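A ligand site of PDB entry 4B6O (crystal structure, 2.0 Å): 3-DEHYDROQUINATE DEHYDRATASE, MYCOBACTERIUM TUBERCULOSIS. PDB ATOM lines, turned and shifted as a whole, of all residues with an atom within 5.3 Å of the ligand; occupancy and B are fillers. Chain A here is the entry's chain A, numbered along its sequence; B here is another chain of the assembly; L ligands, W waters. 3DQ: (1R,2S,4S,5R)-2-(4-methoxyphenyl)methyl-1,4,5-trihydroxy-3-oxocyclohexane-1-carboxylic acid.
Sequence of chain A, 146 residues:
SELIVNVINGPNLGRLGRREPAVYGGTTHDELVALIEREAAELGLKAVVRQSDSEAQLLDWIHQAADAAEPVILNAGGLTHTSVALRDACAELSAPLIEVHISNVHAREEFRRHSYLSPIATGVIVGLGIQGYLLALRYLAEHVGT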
ATOM      1  N   PRO A  11      14.294 -22.559  -8.267  1.00  0.00           N
ATOM      2  CA  PRO A  11      15.574 -22.795  -8.929  1.00  0.00           C
ATOM      3  C   PRO A  11      16.786 -22.522  -8.075  1.00  0.00           C
ATOM      4  O   PRO A  11      16.827 -21.543  -7.319  1.00  0.00           O
ATOM      5  CB  PRO A  11      15.558 -21.816 -10.116  1.00  0.00           C
ATOM      6  CG  PRO A  11      14.138 -21.513 -10.358  1.00  0.00           C
ATOM      7  CD  PRO A  11      13.385 -21.733  -9.085  1.00  0.00           C
ATOM      8  N   ASN A  12      17.776 -23.397  -8.252  1.00  0.00           N
ATOM      9  CA  ASN A  12      19.036 -23.352  -7.570  1.00  0.00           C
ATOM     10  C   ASN A  12      19.036 -23.792  -6.106  1.00  0.00           C
ATOM     11  O   ASN A  12      20.113 -23.979  -5.523  1.00  0.00           O
ATOM     12  CB  ASN A  12      19.695 -22.012  -7.769  1.00  0.00           C
ATOM     13  CG  ASN A  12      19.962 -21.722  -9.240  1.00  0.00           C
ATOM     14  OD1 ASN A  12      20.653 -22.518  -9.908  1.00  0.00           O
ATOM     15  ND2 ASN A  12      19.417 -20.629  -9.758  1.00  0.00           N
ATOM     16  N   LEU A  13      17.873 -23.979  -5.518  1.00  0.00           N
ATOM     17  CA  LEU A  13      17.821 -24.370  -4.123  1.00  0.00           C
ATOM     18  C   LEU A  13      18.390 -25.763  -3.876  1.00  0.00           C
ATOM     19  O   LEU A  13      18.777 -26.088  -2.753  1.00  0.00           O
ATOM     20  CB  LEU A  13      16.417 -24.238  -3.543  1.00  0.00           C
ATOM     21  CG  LEU A  13      16.124 -22.874  -2.879  1.00  0.00           C
ATOM     22  CD1 LEU A  13      17.034 -22.606  -1.628  1.00  0.00           C
ATOM     23  CD2 LEU A  13      16.227 -21.739  -3.907  1.00  0.00           C
ATOM     24  N   ARG A  15      21.146 -26.560  -4.870  1.00  0.00           N
ATOM     25  CA  ARG A  15      22.583 -26.345  -4.812  1.00  0.00           C
ATOM     26  C   ARG A  15      23.124 -26.023  -3.419  1.00  0.00           C
ATOM     27  O   ARG A  15      24.320 -25.777  -3.284  1.00  0.00           O
ATOM     28  CB  ARG A  15      23.003 -25.212  -5.758  1.00  0.00           C
ATOM     29  CG  ARG A  15      22.628 -25.410  -7.225  1.00  0.00           C
ATOM     30  CD  ARG A  15      23.394 -26.562  -7.852  1.00  0.00           C
ATOM     31  NE  ARG A  15      24.816 -26.279  -7.855  1.00  0.00           N
ATOM     32  CZ  ARG A  15      25.758 -27.183  -8.133  1.00  0.00           C
ATOM     33  NH1 ARG A  15      25.432 -28.425  -8.459  1.00  0.00           N
ATOM     34  NH2 ARG A  15      27.034 -26.828  -8.053  1.00  0.00           N
ATOM     35  N   LEU A  16      22.269 -25.967  -2.391  1.00  0.00           N
ATOM     36  CA  LEU A  16      22.736 -25.604  -1.048  1.00  0.00           C
ATOM     37  C   LEU A  16      23.823 -26.581  -0.621  1.00  0.00           C
ATOM     38  O   LEU A  16      23.702 -27.794  -0.873  1.00  0.00           O
ATOM     39  CB  LEU A  16      21.575 -25.662  -0.031  1.00  0.00           C
ATOM     40  CG  LEU A  16      20.426 -24.655  -0.201  1.00  0.00           C
ATOM     41  CD1 LEU A  16      19.194 -25.020   0.669  1.00  0.00           C
ATOM     42  CD2 LEU A  16      20.895 -23.213   0.053  1.00  0.00           C
ATOM     43  N   ARG A  19      28.775 -25.413  -3.060  1.00  0.00           N
ATOM     44  CA  ARG A  19      29.877 -24.445  -3.214  1.00  0.00           C
ATOM     45  C   ARG A  19      30.492 -24.086  -1.862  1.00  0.00           C
ATOM     46  O   ARG A  19      29.811 -24.080  -0.839  1.00  0.00           O
ATOM     47  CB  ARG A  19      29.413 -23.169  -3.937  1.00  0.00           C
ATOM     48  CG  ARG A  19      30.452 -22.032  -3.979  1.00  0.00           C
ATOM     49  CD  ARG A  19      30.045 -20.801  -4.821  1.00  0.00           C
ATOM     50  NE  ARG A  19      28.641 -20.394  -4.630  1.00  0.00           N
ATOM     51  CZ  ARG A  19      28.160 -19.158  -4.839  1.00  0.00           C
ATOM     52  NH1 ARG A  19      28.973 -18.166  -5.232  1.00  0.00           N
ATOM     53  NH2 ARG A  19      26.859 -18.909  -4.650  1.00  0.00           N
ATOM     54  N   TYR A  24      26.618 -20.190   1.347  1.00  0.00           N
ATOM     55  CA  TYR A  24      25.364 -20.896   1.695  1.00  0.00           C
ATOM     56  C   TYR A  24      25.758 -22.388   1.653  1.00  0.00           C
ATOM     57  O   TYR A  24      25.196 -23.204   0.880  1.00  0.00           O
ATOM     58  CB  TYR A  24      24.205 -20.636   0.689  1.00  0.00           C
ATOM     59  CG  TYR A  24      23.915 -19.205   0.186  1.00  0.00           C
ATOM     60  CD1 TYR A  24      24.952 -18.329  -0.146  1.00  0.00           C
ATOM     61  CD2 TYR A  24      22.616 -18.776  -0.008  1.00  0.00           C
ATOM     62  CE1 TYR A  24      24.701 -17.057  -0.617  1.00  0.00           C
ATOM     63  CE2 TYR A  24      22.358 -17.494  -0.499  1.00  0.00           C
ATOM     64  CZ  TYR A  24      23.408 -16.630  -0.799  1.00  0.00           C
ATOM     65  OH  TYR A  24      23.207 -15.349  -1.271  1.00  0.00           O
ATOM     66  N   ASN A  75      10.068 -20.615  -1.178  1.00  0.00           N
ATOM     67  CA  ASN A  75      11.285 -19.945  -1.538  1.00  0.00           C
ATOM     68  C   ASN A  75      11.482 -20.192  -3.028  1.00  0.00           C
ATOM     69  O   ASN A  75      12.022 -21.227  -3.439  1.00  0.00           O
ATOM     70  CB  ASN A  75      12.450 -20.550  -0.776  1.00  0.00           C
ATOM     71  CG  ASN A  75      13.745 -19.829  -1.038  1.00  0.00           C
ATOM     72  OD1 ASN A  75      13.833 -18.971  -1.929  1.00  0.00           O
ATOM     73  ND2 ASN A  75      14.745 -20.107  -0.202  1.00  0.00           N
ATOM     74  N   ALA A  76      11.021 -19.227  -3.825  1.00  0.00           N
ATOM     75  CA  ALA A  76      10.989 -19.378  -5.273  1.00  0.00           C
ATOM     76  C   ALA A  76      12.339 -19.091  -5.943  1.00  0.00           C
ATOM     77  O   ALA A  76      12.410 -19.092  -7.183  1.00  0.00           O
ATOM     78  CB  ALA A  76       9.868 -18.451  -5.861  1.00  0.00           C
ATOM     79  N   GLY A  77      13.394 -18.862  -5.159  1.00  0.00           N
ATOM     80  CA  GLY A  77      14.699 -18.562  -5.738  1.00  0.00           C
ATOM     81  C   GLY A  77      14.642 -17.330  -6.646  1.00  0.00           C
ATOM     82  O   GLY A  77      13.899 -16.401  -6.340  1.00  0.00           O
ATOM     83  N   GLY A  78      15.347 -17.346  -7.773  1.00  0.00           N
ATOM     84  CA  GLY A  78      15.376 -16.197  -8.669  1.00  0.00           C
ATOM     85  C   GLY A  78      13.987 -15.780  -9.214  1.00  0.00           C
ATOM     86  O   GLY A  78      13.774 -14.620  -9.540  1.00  0.00           O
ATOM     87  N   THR A  80      11.375 -15.446  -7.610  1.00  0.00           N
ATOM     88  CA  THR A  80      10.847 -14.435  -6.681  1.00  0.00           C
ATOM     89  C   THR A  80      10.800 -13.042  -7.338  1.00  0.00           C
ATOM     90  O   THR A  80       9.809 -12.299  -7.217  1.00  0.00           O
ATOM     91  CB  THR A  80      11.722 -14.370  -5.432  1.00  0.00           C
ATOM     92  OG1 THR A  80      11.811 -15.708  -4.886  1.00  0.00           O
ATOM     93  CG2 THR A  80      11.116 -13.417  -4.399  1.00  0.00           C
ATOM     94  N   HIS A  81      11.875 -12.732  -8.052  1.00  0.00           N
ATOM     95  CA  HIS A  81      12.133 -11.391  -8.564  1.00  0.00           C
ATOM     96  C   HIS A  81      11.598 -11.190  -9.972  1.00  0.00           C
ATOM     97  O   HIS A  81      11.515 -10.044 -10.410  1.00  0.00           O
ATOM     98  CB  HIS A  81      13.639 -11.097  -8.521  1.00  0.00           C
ATOM     99  CG  HIS A  81      14.278 -11.492  -7.221  1.00  0.00           C
ATOM    100  ND1 HIS A  81      13.919 -10.912  -6.023  1.00  0.00           N
ATOM    101  CD2 HIS A  81      15.193 -12.445  -6.925  1.00  0.00           C
ATOM    102  CE1 HIS A  81      14.613 -11.484  -5.052  1.00  0.00           C
ATOM    103  NE2 HIS A  81      15.382 -12.419  -5.568  1.00  0.00           N
ATOM    104  N   VAL A 100       9.774 -17.371   2.052  1.00  0.00           N
ATOM    105  CA  VAL A 100      11.030 -17.452   2.794  1.00  0.00           C
ATOM    106  C   VAL A 100      12.244 -17.300   1.872  1.00  0.00           C
ATOM    107  O   VAL A 100      12.288 -17.864   0.771  1.00  0.00           O
ATOM    108  CB  VAL A 100      11.126 -18.799   3.596  1.00  0.00           C
ATOM    109  CG1 VAL A 100      12.562 -19.055   4.104  1.00  0.00           C
ATOM    110  CG2 VAL A 100      10.115 -18.813   4.694  1.00  0.00           C
ATOM    111  N   HIS A 101      13.231 -16.514   2.322  1.00  0.00           N
ATOM    112  CA  HIS A 101      14.561 -16.498   1.710  1.00  0.00           C
ATOM    113  C   HIS A 101      15.623 -16.694   2.796  1.00  0.00           C
ATOM    114  O   HIS A 101      15.552 -16.115   3.881  1.00  0.00           O
ATOM    115  CB  HIS A 101      14.780 -15.228   0.906  1.00  0.00           C
ATOM    116  CG  HIS A 101      13.697 -14.981  -0.078  1.00  0.00           C
ATOM    117  ND1 HIS A 101      13.577 -15.713  -1.243  1.00  0.00           N
ATOM    118  CD2 HIS A 101      12.646 -14.137  -0.061  1.00  0.00           C
ATOM    119  CE1 HIS A 101      12.502 -15.316  -1.903  1.00  0.00           C
ATOM    120  NE2 HIS A 101      11.913 -14.356  -1.195  1.00  0.00           N
ATOM    121  N   ILE A 102      16.614 -17.519   2.474  1.00  0.00           N
ATOM    122  CA  ILE A 102      17.724 -17.829   3.358  1.00  0.00           C
ATOM    123  C   ILE A 102      18.579 -16.586   3.540  1.00  0.00           C
ATOM    124  O   ILE A 102      18.828 -16.173   4.675  1.00  0.00           O
ATOM    125  CB  ILE A 102      18.538 -18.996   2.736  1.00  0.00           C
ATOM    126  CG1 ILE A 102      17.643 -20.256   2.686  1.00  0.00           C
ATOM    127  CG2 ILE A 102      19.876 -19.239   3.511  1.00  0.00           C
ATOM    128  CD1 ILE A 102      18.276 -21.424   1.949  1.00  0.00           C
ATOM    129  N   SER A 103      18.964 -15.953   2.434  1.00  0.00           N
ATOM    130  CA  SER A 103      19.785 -14.750   2.464  1.00  0.00           C
ATOM    131  C   SER A 103      18.914 -13.515   2.731  1.00  0.00           C
ATOM    132  O   SER A 103      17.691 -13.550   2.559  1.00  0.00           O
ATOM    133  CB  SER A 103      20.501 -14.581   1.112  1.00  0.00           C
ATOM    134  OG  SER A 103      19.566 -14.153   0.107  1.00  0.00           O
ATOM    135  N   VAL A 105      17.721 -10.611   1.223  1.00  0.00           N
ATOM    136  CA  VAL A 105      17.579 -10.125  -0.140  1.00  0.00           C
ATOM    137  C   VAL A 105      17.674  -8.589  -0.245  1.00  0.00           C
ATOM    138  O   VAL A 105      17.769  -8.061  -1.354  1.00  0.00           O
ATOM    139  CB  VAL A 105      16.254 -10.621  -0.787  1.00  0.00           C
ATOM    140  CG1 VAL A 105      16.212 -12.172  -0.843  1.00  0.00           C
ATOM    141  CG2 VAL A 105      15.008 -10.051  -0.066  1.00  0.00           C
ATOM    142  N   ARG A 108      21.770  -6.836  -0.918  1.00  0.00           N
ATOM    143  CA  ARG A 108      22.503  -7.225  -2.136  1.00  0.00           C
ATOM    144  C   ARG A 108      22.136  -6.271  -3.253  1.00  0.00           C
ATOM    145  O   ARG A 108      22.001  -5.066  -3.004  1.00  0.00           O
ATOM    146  CB  ARG A 108      22.184  -8.692  -2.483  1.00  0.00           C
ATOM    147  CG  ARG A 108      22.378  -9.677  -1.327  1.00  0.00           C
ATOM    148  CD  ARG A 108      22.053 -11.142  -1.727  1.00  0.00           C
ATOM    149  NE  ARG A 108      22.930 -11.553  -2.815  1.00  0.00           N
ATOM    150  CZ  ARG A 108      22.780 -12.662  -3.553  1.00  0.00           C
ATOM    151  NH1 ARG A 108      21.783 -13.514  -3.320  1.00  0.00           N
ATOM    152  NH2 ARG A 108      23.663 -12.917  -4.519  1.00  0.00           N
ATOM    153  N   ARG A 112      17.075  -7.489  -6.255  1.00  0.00           N
ATOM    154  CA  ARG A 112      16.627  -8.502  -5.281  1.00  0.00           C
ATOM    155  C   ARG A 112      15.661  -7.944  -4.200  1.00  0.00           C
ATOM    156  O   ARG A 112      15.009  -8.728  -3.498  1.00  0.00           O
ATOM    157  CB  ARG A 112      17.825  -9.202  -4.636  1.00  0.00           C
ATOM    158  CG  ARG A 112      18.675  -9.987  -5.639  1.00  0.00           C
ATOM    159  CD  ARG A 112      19.803 -10.771  -4.955  1.00  0.00           C
ATOM    160  NE  ARG A 112      20.736 -11.258  -5.957  1.00  0.00           N
ATOM    161  CZ  ARG A 112      20.585 -12.370  -6.670  1.00  0.00           C
ATOM    162  NH1 ARG A 112      19.534 -13.194  -6.484  1.00  0.00           N
ATOM    163  NH2 ARG A 112      21.492 -12.672  -7.568  1.00  0.00           N
ATOM    164  N   VAL B  84      16.923 -13.997 -13.354  1.00  0.00           N
ATOM    165  CA  VAL B  84      17.792 -13.939 -12.168  1.00  0.00           C
ATOM    166  C   VAL B  84      18.250 -15.355 -11.801  1.00  0.00           C
ATOM    167  O   VAL B  84      19.360 -15.546 -11.398  1.00  0.00           O
ATOM    168  CB  VAL B  84      17.078 -13.259 -10.948  1.00  0.00           C
ATOM    169  CG1 VAL B  84      17.905 -13.402  -9.695  1.00  0.00           C
ATOM    170  CG2 VAL B  84      16.806 -11.784 -11.242  1.00  0.00           C
ATOM    171  N   ASP B  88      22.028 -16.463 -10.840  1.00  0.00           N
ATOM    172  CA  ASP B  88      22.351 -17.171  -9.589  1.00  0.00           C
ATOM    173  C   ASP B  88      23.206 -18.422  -9.859  1.00  0.00           C
ATOM    174  O   ASP B  88      24.182 -18.691  -9.155  1.00  0.00           O
ATOM    175  CB  ASP B  88      21.087 -17.643  -8.852  1.00  0.00           C
ATOM    176  CG  ASP B  88      20.223 -16.498  -8.296  1.00  0.00           C
ATOM    177  OD1 ASP B  88      20.781 -15.422  -8.010  1.00  0.00           O
ATOM    178  OD2 ASP B  88      18.998 -16.730  -8.129  1.00  0.00           O
ATOM    179  N   ALA B  89      22.792 -19.229 -10.831  1.00  0.00           N
ATOM    180  CA  ALA B  89      23.540 -20.435 -11.206  1.00  0.00           C
ATOM    181  C   ALA B  89      24.947 -20.080 -11.765  1.00  0.00           C
ATOM    182  O   ALA B  89      25.939 -20.702 -11.409  1.00  0.00           O
ATOM    183  CB  ALA B  89      22.764 -21.261 -12.216  1.00  0.00           C
ATOM    184  N   GLU B  92      27.937 -19.187  -9.468  1.00  0.00           N
ATOM    185  CA  GLU B  92      28.640 -20.337  -8.866  1.00  0.00           C
ATOM    186  C   GLU B  92      29.881 -20.772  -9.626  1.00  0.00           C
ATOM    187  O   GLU B  92      30.699 -21.475  -9.086  1.00  0.00           O
ATOM    188  CB  GLU B  92      27.714 -21.568  -8.780  1.00  0.00           C
ATOM    189  CG  GLU B  92      27.332 -22.031  -7.401  1.00  0.00           C
ATOM    190  CD  GLU B  92      26.746 -23.426  -7.413  1.00  0.00           C
ATOM    191  OE1 GLU B  92      25.724 -23.639  -8.082  1.00  0.00           O
ATOM    192  OE2 GLU B  92      27.335 -24.338  -6.789  1.00  0.00           O
HETATM  193  CAA 3DQ L   1      23.541 -21.165  -6.726  1.00  0.00           C
HETATM  194  OAN 3DQ L   1      22.489 -21.566  -5.805  1.00  0.00           O
HETATM  195  CAR 3DQ L   1      21.808 -20.599  -5.111  1.00  0.00           C
HETATM  196  CAK 3DQ L   1      21.967 -19.242  -5.340  1.00  0.00           C
HETATM  197  CAI 3DQ L   1      21.240 -18.306  -4.612  1.00  0.00           C
HETATM  198  CAJ 3DQ L   1      20.903 -21.005  -4.140  1.00  0.00           C
HETATM  199  CAH 3DQ L   1      20.177 -20.076  -3.405  1.00  0.00           C
HETATM  200  CAQ 3DQ L   1      20.364 -18.714  -3.640  1.00  0.00           C
HETATM  201  CAL 3DQ L   1      19.569 -17.716  -2.830  1.00  0.00           C
HETATM  202  CAU 3DQ L   1      18.074 -17.751  -3.207  1.00  0.00           C
HETATM  203  CAP 3DQ L   1      17.917 -17.335  -4.679  1.00  0.00           C
HETATM  204  OAC 3DQ L   1      17.711 -18.177  -5.583  1.00  0.00           O
HETATM  205  CAT 3DQ L   1      18.058 -15.845  -5.005  1.00  0.00           C
HETATM  206  OAF 3DQ L   1      17.697 -15.567  -6.378  1.00  0.00           O
HETATM  207  CAS 3DQ L   1      17.154 -15.042  -4.059  1.00  0.00           C
HETATM  208  OAE 3DQ L   1      17.386 -13.648  -4.288  1.00  0.00           O
HETATM  209  CAM 3DQ L   1      17.467 -15.356  -2.586  1.00  0.00           C
HETATM  210  CAV 3DQ L   1      17.171 -16.840  -2.282  1.00  0.00           C
HETATM  211  CAO 3DQ L   1      17.432 -17.186  -0.803  1.00  0.00           C
HETATM  212  OAB 3DQ L   1      18.226 -16.455  -0.146  1.00  0.00           O
HETATM  213  OAD 3DQ L   1      16.822 -18.190  -0.334  1.00  0.00           O
HETATM  214  OAG 3DQ L   1      15.768 -17.085  -2.615  1.00  0.00           O
HETATM  215  O   HOH W   1      19.475 -12.795  -2.303  1.00  0.00           O
HETATM  216  O   HOH W   2      22.499 -15.412  -5.866  1.00  0.00           O
HETATM  217  O   HOH W   3      17.573 -19.010  -8.299  1.00  0.00           O
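An oxygen (OAF) of the ligand is in hydrogen-bond range of the backbone NH (N) of Gly 78 (3.3 Å).
NE2 of His 81 is in hydrogen-bond range of OAE of the ligand, 2.7 Å away.
OAD of the ligand is in hydrogen-bond range of N of Ile 102.
The side-chain hydroxyl (OG) of Ser 103 is in hydrogen-bond range of an oxygen (OAB) of the ligand, 2.7 Å away.
A ring nitrogen (ND1) of His 101 sits at hydrogen-bond distance from an oxygen (OAG) of the ligand.
NH1 of Arg 112 sits at hydrogen-bond distance from OAF of the ligand (3.0 Å).
An oxygen (OAF) of the ligand lies within hydrogen-bond range of the side-chain carboxylate of Asp 88 of chain B.
An oxygen (OAB) of the ligand sits at hydrogen-bond distance from the backbone NH of Ser 103.
The side-chain amide oxygen (OD1) of Asn 75 sits at hydrogen-bond distance from an oxygen (OAG) of the ligand.
OG1 of Thr 80 is in hydrogen-bond range of O of Gly 77, 2.6 Å away.
NE of Arg 15 lies within salt-bridge range of OE1 of Glu 92 of chain B (2.8 Å).
NH2 of Arg 112 lies within salt-bridge range of OD1 of Asp 88 of chain B.
The backbone carbonyl oxygen (O) of Val 100 sits close to the side-chain amide oxygen (OD1) of Asn 75, 3.3 Å away.
The side-chain amide oxygen (OD1) of Asn 75 lies close to the backbone NH (N) of Gly 77.
The side-chain amide oxygen (OD1) of Asn 75 lies within hydrogen-bond range of a ring nitrogen (ND1) of His 101.
The side-chain hydroxyl (OH) of Tyr 24 sits at hydrogen-bond distance from the guanidinium group (NH1) of Arg 108 (3.1 Å).
The backbone carbonyl oxygen (O) of Asn 12 sits close to an oxygen (OAN) of the ligand (3.4 Å).
O of Pro 11 touches OAC of the ligand, 3.9 Å away.
Arg 15 touches the ligand (CB to OAN, 3.7 Å).
Tyr 24 touches the ligand.
CA of Gly 77 touches OAC of the ligand, at 3.0 Å.
Val 105 touches the ligand (CG1 to CAM, 3.8 Å).
Val 84 of chain B touches the ligand (CG1 to OAF, 3.97 Å).
Glu 92 of chain B touches the ligand (OE1 to CAA, 3.6 Å).
Of the 24 residues printed, 16 come within 4 Å of the ligand.
The nearest printed residue that does not touch the ligand is Leu 13 (4.2 Å).
Water W1 lies within hydrogen-bond range of NH1 of Arg 108 (2.6 Å), OG of Ser 103 (2.8 Å) and OAE of the ligand (3.0 Å).
Water W2 lies within hydrogen-bond range of OD1 of Asp 88 of chain B (2.7 Å), NH2 of Arg 108 (3.1 Å) and NH2 of Arg 112 (3.4 Å).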
